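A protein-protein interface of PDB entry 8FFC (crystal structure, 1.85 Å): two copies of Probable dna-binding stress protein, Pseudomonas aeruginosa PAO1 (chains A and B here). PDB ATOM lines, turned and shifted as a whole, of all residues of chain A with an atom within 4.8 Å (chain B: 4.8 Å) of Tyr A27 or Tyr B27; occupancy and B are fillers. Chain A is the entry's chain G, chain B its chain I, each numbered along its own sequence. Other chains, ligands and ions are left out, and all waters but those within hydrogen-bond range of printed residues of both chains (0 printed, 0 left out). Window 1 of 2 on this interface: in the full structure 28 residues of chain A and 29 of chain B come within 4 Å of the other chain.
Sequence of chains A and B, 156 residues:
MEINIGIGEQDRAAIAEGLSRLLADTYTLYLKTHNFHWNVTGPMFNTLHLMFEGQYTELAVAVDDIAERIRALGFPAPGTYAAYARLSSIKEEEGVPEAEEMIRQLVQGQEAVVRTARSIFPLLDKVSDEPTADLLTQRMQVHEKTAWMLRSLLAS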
ATOM      1  N   LEU A  23      12.239  -2.707 -14.630  1.00  0.00           N
ATOM      2  CA  LEU A  23      12.545  -4.089 -15.000  1.00  0.00           C
ATOM      3  C   LEU A  23      12.040  -5.050 -13.934  1.00  0.00           C
ATOM      4  O   LEU A  23      11.397  -6.048 -14.239  1.00  0.00           O
ATOM      5  CB  LEU A  23      14.049  -4.234 -15.197  1.00  0.00           C
ATOM      6  CG  LEU A  23      14.602  -5.635 -15.527  1.00  0.00           C
ATOM      7  CD1 LEU A  23      14.007  -6.147 -16.778  1.00  0.00           C
ATOM      8  CD2 LEU A  23      16.090  -5.569 -15.639  1.00  0.00           C
ATOM      9  N   ALA A  24      12.306  -4.742 -12.664  1.00  0.00           N
ATOM     10  CA  ALA A  24      11.847  -5.603 -11.575  1.00  0.00           C
ATOM     11  C   ALA A  24      10.329  -5.734 -11.564  1.00  0.00           C
ATOM     12  O   ALA A  24       9.792  -6.840 -11.414  1.00  0.00           O
ATOM     13  CB  ALA A  24      12.349  -5.064 -10.244  1.00  0.00           C
ATOM     14  N   ASP A  25       9.610  -4.619 -11.687  1.00  0.00           N
ATOM     15  CA  ASP A  25       8.158  -4.697 -11.734  1.00  0.00           C
ATOM     16  C   ASP A  25       7.694  -5.528 -12.918  1.00  0.00           C
ATOM     17  O   ASP A  25       6.741  -6.313 -12.808  1.00  0.00           O
ATOM     18  CB  ASP A  25       7.535  -3.304 -11.846  1.00  0.00           C
ATOM     19  CG  ASP A  25       7.601  -2.520 -10.546  1.00  0.00           C
ATOM     20  OD1 ASP A  25       7.967  -3.106  -9.521  1.00  0.00           O
ATOM     21  OD2 ASP A  25       7.273  -1.327 -10.561  1.00  0.00           O
ATOM     22  N   THR A  26       8.327  -5.328 -14.072  1.00  0.00           N
ATOM     23  CA  THR A  26       7.874  -6.026 -15.262  1.00  0.00           C
ATOM     24  C   THR A  26       8.145  -7.518 -15.142  1.00  0.00           C
ATOM     25  O   THR A  26       7.315  -8.343 -15.550  1.00  0.00           O
ATOM     26  CB  THR A  26       8.565  -5.449 -16.491  1.00  0.00           C
ATOM     27  OG1 THR A  26       8.249  -4.047 -16.592  1.00  0.00           O
ATOM     28  CG2 THR A  26       8.130  -6.150 -17.774  1.00  0.00           C
ATOM     29  N   TYR A  27       9.308  -7.876 -14.605  1.00  0.00           N
ATOM     30  CA  TYR A  27       9.613  -9.292 -14.471  1.00  0.00           C
ATOM     31  C   TYR A  27       8.709  -9.939 -13.434  1.00  0.00           C
ATOM     32  O   TYR A  27       8.268 -11.082 -13.603  1.00  0.00           O
ATOM     33  CB  TYR A  27      11.080  -9.493 -14.096  1.00  0.00           C
ATOM     34  CG  TYR A  27      11.481 -10.899 -14.348  1.00  0.00           C
ATOM     35  CD1 TYR A  27      11.203 -11.900 -13.408  1.00  0.00           C
ATOM     36  CD2 TYR A  27      12.072 -11.252 -15.552  1.00  0.00           C
ATOM     37  CE1 TYR A  27      11.534 -13.207 -13.646  1.00  0.00           C
ATOM     38  CE2 TYR A  27      12.411 -12.564 -15.816  1.00  0.00           C
ATOM     39  CZ  TYR A  27      12.142 -13.540 -14.864  1.00  0.00           C
ATOM     40  OH  TYR A  27      12.481 -14.851 -15.128  1.00  0.00           O
ATOM     41  N   THR A  28       8.409  -9.220 -12.353  1.00  0.00           N
ATOM     42  CA  THR A  28       7.514  -9.782 -11.347  1.00  0.00           C
ATOM     43  C   THR A  28       6.122  -9.978 -11.923  1.00  0.00           C
ATOM     44  O   THR A  28       5.489 -11.013 -11.686  1.00  0.00           O
ATOM     45  CB  THR A  28       7.476  -8.895 -10.099  1.00  0.00           C
ATOM     46  OG1 THR A  28       8.818  -8.687  -9.607  1.00  0.00           O
ATOM     47  CG2 THR A  28       6.633  -9.556  -9.026  1.00  0.00           C
ATOM     48  N   LEU A  29       5.642  -9.018 -12.733  1.00  0.00           N
ATOM     49  CA  LEU A  29       4.356  -9.184 -13.398  1.00  0.00           C
ATOM     50  C   LEU A  29       4.384 -10.333 -14.407  1.00  0.00           C
ATOM     51  O   LEU A  29       3.398 -11.052 -14.558  1.00  0.00           O
ATOM     52  CB  LEU A  29       3.938  -7.878 -14.105  1.00  0.00           C
ATOM     53  CG  LEU A  29       2.529  -7.818 -14.683  1.00  0.00           C
ATOM     54  CD1 LEU A  29       1.437  -8.129 -13.700  1.00  0.00           C
ATOM     55  CD2 LEU A  29       2.284  -6.457 -15.318  1.00  0.00           C
ATOM     56  N   TYR A  30       5.495 -10.494 -15.120  1.00  0.00           N
ATOM     57  CA  TYR A  30       5.653 -11.614 -16.047  1.00  0.00           C
ATOM     58  C   TYR A  30       5.462 -12.957 -15.337  1.00  0.00           C
ATOM     59  O   TYR A  30       4.677 -13.804 -15.781  1.00  0.00           O
ATOM     60  CB  TYR A  30       7.032 -11.508 -16.675  1.00  0.00           C
ATOM     61  CG  TYR A  30       7.560 -12.741 -17.366  1.00  0.00           C
ATOM     62  CD1 TYR A  30       6.997 -13.190 -18.543  1.00  0.00           C
ATOM     63  CD2 TYR A  30       8.640 -13.435 -16.852  1.00  0.00           C
ATOM     64  CE1 TYR A  30       7.482 -14.298 -19.189  1.00  0.00           C
ATOM     65  CE2 TYR A  30       9.130 -14.572 -17.488  1.00  0.00           C
ATOM     66  CZ  TYR A  30       8.550 -14.994 -18.667  1.00  0.00           C
ATOM     67  OH  TYR A  30       9.039 -16.109 -19.325  1.00  0.00           O
ATOM     68  N   LEU A  31       6.176 -13.170 -14.231  1.00  0.00           N
ATOM     69  CA  LEU A  31       6.044 -14.432 -13.502  1.00  0.00           C
ATOM     70  C   LEU A  31       4.643 -14.617 -12.919  1.00  0.00           C
ATOM     71  O   LEU A  31       4.092 -15.715 -12.988  1.00  0.00           O
ATOM     72  CB  LEU A  31       7.116 -14.523 -12.415  1.00  0.00           C
ATOM     73  CG  LEU A  31       7.083 -15.789 -11.543  1.00  0.00           C
ATOM     74  CD1 LEU A  31       7.173 -17.032 -12.396  1.00  0.00           C
ATOM     75  CD2 LEU A  31       8.218 -15.750 -10.524  1.00  0.00           C
ATOM     76  N   VAL A  63      10.894  -7.346 -20.889  1.00  0.00           N
ATOM     77  CA  VAL A  63      12.003  -7.513 -19.947  1.00  0.00           C
ATOM     78  C   VAL A  63      13.328  -7.375 -20.681  1.00  0.00           C
ATOM     79  O   VAL A  63      14.276  -6.738 -20.210  1.00  0.00           O
ATOM     80  CB  VAL A  63      11.876  -8.881 -19.239  1.00  0.00           C
ATOM     81  CG1 VAL A  63      13.201  -9.361 -18.671  1.00  0.00           C
ATOM     82  CG2 VAL A  63      10.816  -8.806 -18.155  1.00  0.00           C
ATOM     83  N   TYR A  81      16.345 -13.202  -8.333  1.00  0.00           N
ATOM     84  CA  TYR A  81      15.177 -13.089  -7.474  1.00  0.00           C
ATOM     85  C   TYR A  81      15.362 -12.020  -6.400  1.00  0.00           C
ATOM     86  O   TYR A  81      14.428 -11.266  -6.111  1.00  0.00           O
ATOM     87  CB  TYR A  81      14.872 -14.422  -6.789  1.00  0.00           C
ATOM     88  CG  TYR A  81      14.633 -15.625  -7.707  1.00  0.00           C
ATOM     89  CD1 TYR A  81      14.041 -15.479  -8.959  1.00  0.00           C
ATOM     90  CD2 TYR A  81      15.010 -16.900  -7.307  1.00  0.00           C
ATOM     91  CE1 TYR A  81      13.823 -16.584  -9.790  1.00  0.00           C
ATOM     92  CE2 TYR A  81      14.813 -18.009  -8.136  1.00  0.00           C
ATOM     93  CZ  TYR A  81      14.205 -17.837  -9.365  1.00  0.00           C
ATOM     94  OH  TYR A  81      14.012 -18.929 -10.177  1.00  0.00           O
ATOM     95  N   TYR A  84      15.206  -8.464  -7.854  1.00  0.00           N
ATOM     96  CA  TYR A  84      13.869  -8.067  -8.254  1.00  0.00           C
ATOM     97  C   TYR A  84      12.954  -7.903  -7.042  1.00  0.00           C
ATOM     98  O   TYR A  84      12.150  -6.972  -6.998  1.00  0.00           O
ATOM     99  CB  TYR A  84      13.280  -9.071  -9.253  1.00  0.00           C
ATOM    100  CG  TYR A  84      13.961  -9.072 -10.617  1.00  0.00           C
ATOM    101  CD1 TYR A  84      14.819  -8.051 -11.003  1.00  0.00           C
ATOM    102  CD2 TYR A  84      13.740 -10.123 -11.531  1.00  0.00           C
ATOM    103  CE1 TYR A  84      15.437  -8.063 -12.266  1.00  0.00           C
ATOM    104  CE2 TYR A  84      14.356 -10.134 -12.794  1.00  0.00           C
ATOM    105  CZ  TYR A  84      15.175  -9.111 -13.156  1.00  0.00           C
ATOM    106  OH  TYR A  84      15.800  -9.128 -14.393  1.00  0.00           O
ATOM    107  N   LEU B  23      11.048 -27.677 -11.894  1.00  0.00           N
ATOM    108  CA  LEU B  23      10.560 -26.390 -12.403  1.00  0.00           C
ATOM    109  C   LEU B  23      11.342 -25.240 -11.803  1.00  0.00           C
ATOM    110  O   LEU B  23      11.781 -24.330 -12.517  1.00  0.00           O
ATOM    111  CB  LEU B  23       9.072 -26.230 -12.090  1.00  0.00           C
ATOM    112  CG  LEU B  23       8.356 -24.918 -12.475  1.00  0.00           C
ATOM    113  CD1 LEU B  23       8.509 -24.690 -13.963  1.00  0.00           C
ATOM    114  CD2 LEU B  23       6.891 -24.934 -12.105  1.00  0.00           C
ATOM    115  N   ALA B  24      11.570 -25.283 -10.484  1.00  0.00           N
ATOM    116  CA  ALA B  24      12.344 -24.222  -9.844  1.00  0.00           C
ATOM    117  C   ALA B  24      13.768 -24.164 -10.385  1.00  0.00           C
ATOM    118  O   ALA B  24      14.303 -23.079 -10.643  1.00  0.00           O
ATOM    119  CB  ALA B  24      12.350 -24.420  -8.326  1.00  0.00           C
ATOM    120  N   ASP B  25      14.420 -25.309 -10.539  1.00  0.00           N
ATOM    121  CA  ASP B  25      15.764 -25.289 -11.107  1.00  0.00           C
ATOM    122  C   ASP B  25      15.760 -24.782 -12.550  1.00  0.00           C
ATOM    123  O   ASP B  25      16.634 -23.997 -12.947  1.00  0.00           O
ATOM    124  CB  ASP B  25      16.374 -26.679 -11.046  1.00  0.00           C
ATOM    125  CG  ASP B  25      16.823 -27.032  -9.653  1.00  0.00           C
ATOM    126  OD1 ASP B  25      17.084 -26.092  -8.869  1.00  0.00           O
ATOM    127  OD2 ASP B  25      16.899 -28.240  -9.351  1.00  0.00           O
ATOM    128  N   THR B  26      14.772 -25.199 -13.337  1.00  0.00           N
ATOM    129  CA  THR B  26      14.707 -24.779 -14.732  1.00  0.00           C
ATOM    130  C   THR B  26      14.474 -23.282 -14.824  1.00  0.00           C
ATOM    131  O   THR B  26      15.126 -22.595 -15.617  1.00  0.00           O
ATOM    132  CB  THR B  26      13.618 -25.551 -15.469  1.00  0.00           C
ATOM    133  OG1 THR B  26      13.913 -26.942 -15.398  1.00  0.00           O
ATOM    134  CG2 THR B  26      13.595 -25.193 -16.929  1.00  0.00           C
ATOM    135  N   TYR B  27      13.594 -22.751 -13.975  1.00  0.00           N
ATOM    136  CA  TYR B  27      13.310 -21.318 -14.008  1.00  0.00           C
ATOM    137  C   TYR B  27      14.503 -20.498 -13.498  1.00  0.00           C
ATOM    138  O   TYR B  27      14.817 -19.430 -14.047  1.00  0.00           O
ATOM    139  CB  TYR B  27      12.060 -21.015 -13.194  1.00  0.00           C
ATOM    140  CG  TYR B  27      11.514 -19.678 -13.553  1.00  0.00           C
ATOM    141  CD1 TYR B  27      12.062 -18.511 -12.983  1.00  0.00           C
ATOM    142  CD2 TYR B  27      10.507 -19.559 -14.503  1.00  0.00           C
ATOM    143  CE1 TYR B  27      11.591 -17.261 -13.331  1.00  0.00           C
ATOM    144  CE2 TYR B  27      10.025 -18.302 -14.882  1.00  0.00           C
ATOM    145  CZ  TYR B  27      10.566 -17.164 -14.283  1.00  0.00           C
ATOM    146  OH  TYR B  27      10.096 -15.924 -14.640  1.00  0.00           O
ATOM    147  N   THR B  28      15.189 -20.989 -12.468  1.00  0.00           N
ATOM    148  CA  THR B  28      16.385 -20.313 -11.983  1.00  0.00           C
ATOM    149  C   THR B  28      17.465 -20.279 -13.060  1.00  0.00           C
ATOM    150  O   THR B  28      18.109 -19.247 -13.285  1.00  0.00           O
ATOM    151  CB  THR B  28      16.884 -20.995 -10.702  1.00  0.00           C
ATOM    152  OG1 THR B  28      15.852 -20.932  -9.713  1.00  0.00           O
ATOM    153  CG2 THR B  28      18.104 -20.286 -10.148  1.00  0.00           C
ATOM    154  N   LEU B  29      17.670 -21.394 -13.756  1.00  0.00           N
ATOM    155  CA  LEU B  29      18.623 -21.412 -14.867  1.00  0.00           C
ATOM    156  C   LEU B  29      18.188 -20.486 -16.000  1.00  0.00           C
ATOM    157  O   LEU B  29      19.016 -19.817 -16.627  1.00  0.00           O
ATOM    158  CB  LEU B  29      18.785 -22.846 -15.370  1.00  0.00           C
ATOM    159  CG  LEU B  29      19.788 -23.091 -16.485  1.00  0.00           C
ATOM    160  CD1 LEU B  29      21.202 -22.629 -16.067  1.00  0.00           C
ATOM    161  CD2 LEU B  29      19.836 -24.556 -16.927  1.00  0.00           C
ATOM    162  N   TYR B  30      16.895 -20.448 -16.286  1.00  0.00           N
ATOM    163  CA  TYR B  30      16.343 -19.484 -17.244  1.00  0.00           C
ATOM    164  C   TYR B  30      16.725 -18.037 -16.909  1.00  0.00           C
ATOM    165  O   TYR B  30      17.204 -17.278 -17.767  1.00  0.00           O
ATOM    166  CB  TYR B  30      14.834 -19.655 -17.244  1.00  0.00           C
ATOM    167  CG  TYR B  30      14.051 -18.589 -17.974  1.00  0.00           C
ATOM    168  CD1 TYR B  30      14.043 -18.530 -19.377  1.00  0.00           C
ATOM    169  CD2 TYR B  30      13.276 -17.672 -17.280  1.00  0.00           C
ATOM    170  CE1 TYR B  30      13.304 -17.560 -20.057  1.00  0.00           C
ATOM    171  CE2 TYR B  30      12.535 -16.696 -17.961  1.00  0.00           C
ATOM    172  CZ  TYR B  30      12.557 -16.651 -19.355  1.00  0.00           C
ATOM    173  OH  TYR B  30      11.821 -15.692 -20.045  1.00  0.00           O
ATOM    174  N   LEU B  31      16.482 -17.617 -15.672  1.00  0.00           N
ATOM    175  CA  LEU B  31      16.808 -16.238 -15.321  1.00  0.00           C
ATOM    176  C   LEU B  31      18.315 -16.011 -15.338  1.00  0.00           C
ATOM    177  O   LEU B  31      18.774 -14.966 -15.815  1.00  0.00           O
ATOM    178  CB  LEU B  31      16.193 -15.883 -13.970  1.00  0.00           C
ATOM    179  CG  LEU B  31      16.436 -14.458 -13.473  1.00  0.00           C
ATOM    180  CD1 LEU B  31      15.960 -13.472 -14.517  1.00  0.00           C
ATOM    181  CD2 LEU B  31      15.719 -14.192 -12.148  1.00  0.00           C
ATOM    182  N   VAL B  63       9.809 -24.537 -19.029  1.00  0.00           N
ATOM    183  CA  VAL B  63       9.123 -24.125 -17.803  1.00  0.00           C
ATOM    184  C   VAL B  63       7.618 -24.351 -17.934  1.00  0.00           C
ATOM    185  O   VAL B  63       6.955 -24.884 -17.037  1.00  0.00           O
ATOM    186  CB  VAL B  63       9.479 -22.653 -17.506  1.00  0.00           C
ATOM    187  CG1 VAL B  63       8.391 -21.949 -16.738  1.00  0.00           C
ATOM    188  CG2 VAL B  63      10.839 -22.576 -16.778  1.00  0.00           C
ATOM    189  N   TYR B  81       8.973 -15.905  -6.727  1.00  0.00           N
ATOM    190  CA  TYR B  81      10.369 -15.881  -6.312  1.00  0.00           C
ATOM    191  C   TYR B  81      10.586 -16.700  -5.049  1.00  0.00           C
ATOM    192  O   TYR B  81      11.595 -17.406  -4.931  1.00  0.00           O
ATOM    193  CB  TYR B  81      10.843 -14.452  -6.042  1.00  0.00           C
ATOM    194  CG  TYR B  81      10.721 -13.494  -7.189  1.00  0.00           C
ATOM    195  CD1 TYR B  81      10.933 -13.899  -8.494  1.00  0.00           C
ATOM    196  CD2 TYR B  81      10.406 -12.169  -6.957  1.00  0.00           C
ATOM    197  CE1 TYR B  81      10.821 -13.003  -9.548  1.00  0.00           C
ATOM    198  CE2 TYR B  81      10.289 -11.260  -8.000  1.00  0.00           C
ATOM    199  CZ  TYR B  81      10.507 -11.679  -9.287  1.00  0.00           C
ATOM    200  OH  TYR B  81      10.401 -10.770 -10.325  1.00  0.00           O
ATOM    201  N   TYR B  84      10.394 -20.488  -5.787  1.00  0.00           N
ATOM    202  CA  TYR B  84      11.513 -21.006  -6.573  1.00  0.00           C
ATOM    203  C   TYR B  84      12.819 -20.951  -5.789  1.00  0.00           C
ATOM    204  O   TYR B  84      13.665 -21.840  -5.927  1.00  0.00           O
ATOM    205  CB  TYR B  84      11.640 -20.236  -7.882  1.00  0.00           C
ATOM    206  CG  TYR B  84      10.551 -20.508  -8.861  1.00  0.00           C
ATOM    207  CD1 TYR B  84       9.702 -21.613  -8.736  1.00  0.00           C
ATOM    208  CD2 TYR B  84      10.350 -19.650  -9.936  1.00  0.00           C
ATOM    209  CE1 TYR B  84       8.698 -21.842  -9.670  1.00  0.00           C
ATOM    210  CE2 TYR B  84       9.372 -19.878 -10.851  1.00  0.00           C
ATOM    211  CZ  TYR B  84       8.555 -20.967 -10.727  1.00  0.00           C
ATOM    212  OH  TYR B  84       7.565 -21.179 -11.644  1.00  0.00           O
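OG1 of Thr A28 lies within hydrogen-bond range of O of Ala A24 (2.8 Å). The backbone carbonyl oxygen (O) of Ala B24 is in hydrogen-bond range of the side-chain hydroxyl (OG1) of Thr B28 (2.8 Å).
Tyr A27 touches Tyr B30 (OH to CE2, 3.4 Å). CD1 of Leu B31 touches OH of Tyr A27, at 3.8 Å. OH of Tyr B81 touches CD1 of Tyr A27 (3.4 Å). Tyr B81 touches Leu A31 (CD1 to CD2, 3.9 Å). Leu A31 touches Tyr B84. OH of Tyr A81 touches CD1 of Tyr B27, 3.4 Å away. Leu B31 touches Tyr A81 (CD2 to CD1, 3.8 Å). CD1 of Tyr A81 touches CD1 of Tyr B81 (3.5 Å). OH of Tyr A81 touches CB of Tyr B84 (3.5 Å). Tyr A84 touches Tyr B81 (CB to OH, 3.5 Å).
Printed residues of chain B that touch a printed residue of chain A: Tyr B27, Thr B28, Tyr B30, Leu B31, Tyr B81 and Tyr B84. Hydrophobic or aromatic side chains of chain B that line the printed part of chain A: Tyr B27, Tyr B30, Leu B31, Tyr B81 and Tyr B84. Of the 12 printed residues of chain A, 6 touch a printed residue of chain B. Printed residues of chain A that touch a printed residue of chain B: Tyr A27, Thr A28, Tyr A30, Leu A31, Tyr A81 and Tyr A84. Hydrophobic or aromatic side chains of chain A within 4 Å of the printed part of chain B: Tyr A27, Tyr A30, Leu A31, Tyr A81 and Tyr A84. Along chain A the printed residues that touch a printed residue of chain B span positions 27 to 84. Among the printed residues, no Asp or Glu carboxylate lies within 4 Å of a Lys or Arg side-chain nitrogen of the other chain.
OH of Tyr A30 lies within hydrogen-bond range of OH of Tyr B30. The side-chain hydroxyl of Tyr A27 is in hydrogen-bond range of the side-chain hydroxyl of Tyr B27, at 2.7 Å. OG1 of Thr A28 is in hydrogen-bond range of OH of Tyr B81, at 2.7 Å. The side-chain hydroxyl (OG1) of Thr B28 lies within hydrogen-bond range of the side-chain hydroxyl (OH) of Tyr A81, 2.8 Å away.
Of the printed residues of chain B, Tyr A27 touches Tyr B27, Tyr B30, Leu B31 and Tyr B81. Of the printed residues of chain B, Tyr A30 touches Tyr B27 and Tyr B30. Printed residues of chain B within 4 Å of Leu A31: Tyr B27 (3.8 Å), Tyr B81 (3.9 Å) and Tyr B84 (3.9 Å). Val A63 touches none of the printed residues of chain B. Of the printed residues of chain B, Tyr A81 touches Tyr B27 (3.4 Å), Thr B28 (2.8 Å), Leu B31 (3.8 Å), Tyr B81 (3.5 Å) and Tyr B84 (3.5 Å). Of chain A, only Tyr A27 (2.7 Å), Tyr A30 (3.3 Å), Leu A31 (3.8 Å) and Tyr A81 (3.4 Å) come within 4 Å of Tyr B27. Of the printed residues of chain A, Thr B28 touches Tyr A81. Of the printed residues of chain A, Tyr B30 touches Tyr A27 (3.4 Å) and Tyr A30 (2.9 Å). The nearest printed residue of chain A that does not touch Tyr B27 is Thr A28 (7.3 Å).
Tyr A27 touches its own counterpart, Tyr B27. Tyr A27 touches Leu B31, and with the chains exchanged Leu A31 touches Tyr B27. Tyr B30 touches its own counterpart, Tyr A30. Leu A31 touches Tyr B84, but with the chains exchanged Tyr A84 does not touch Leu B31 (4.1 Å). Positions printed for both chains: 23, 24, 25, 26, 27, 28, 29, 30, 31, 63, 81 and 84. Of the 16 pairs that touch across the chains among the printed residues, 15 have their exchanged pair printed and touching as well.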
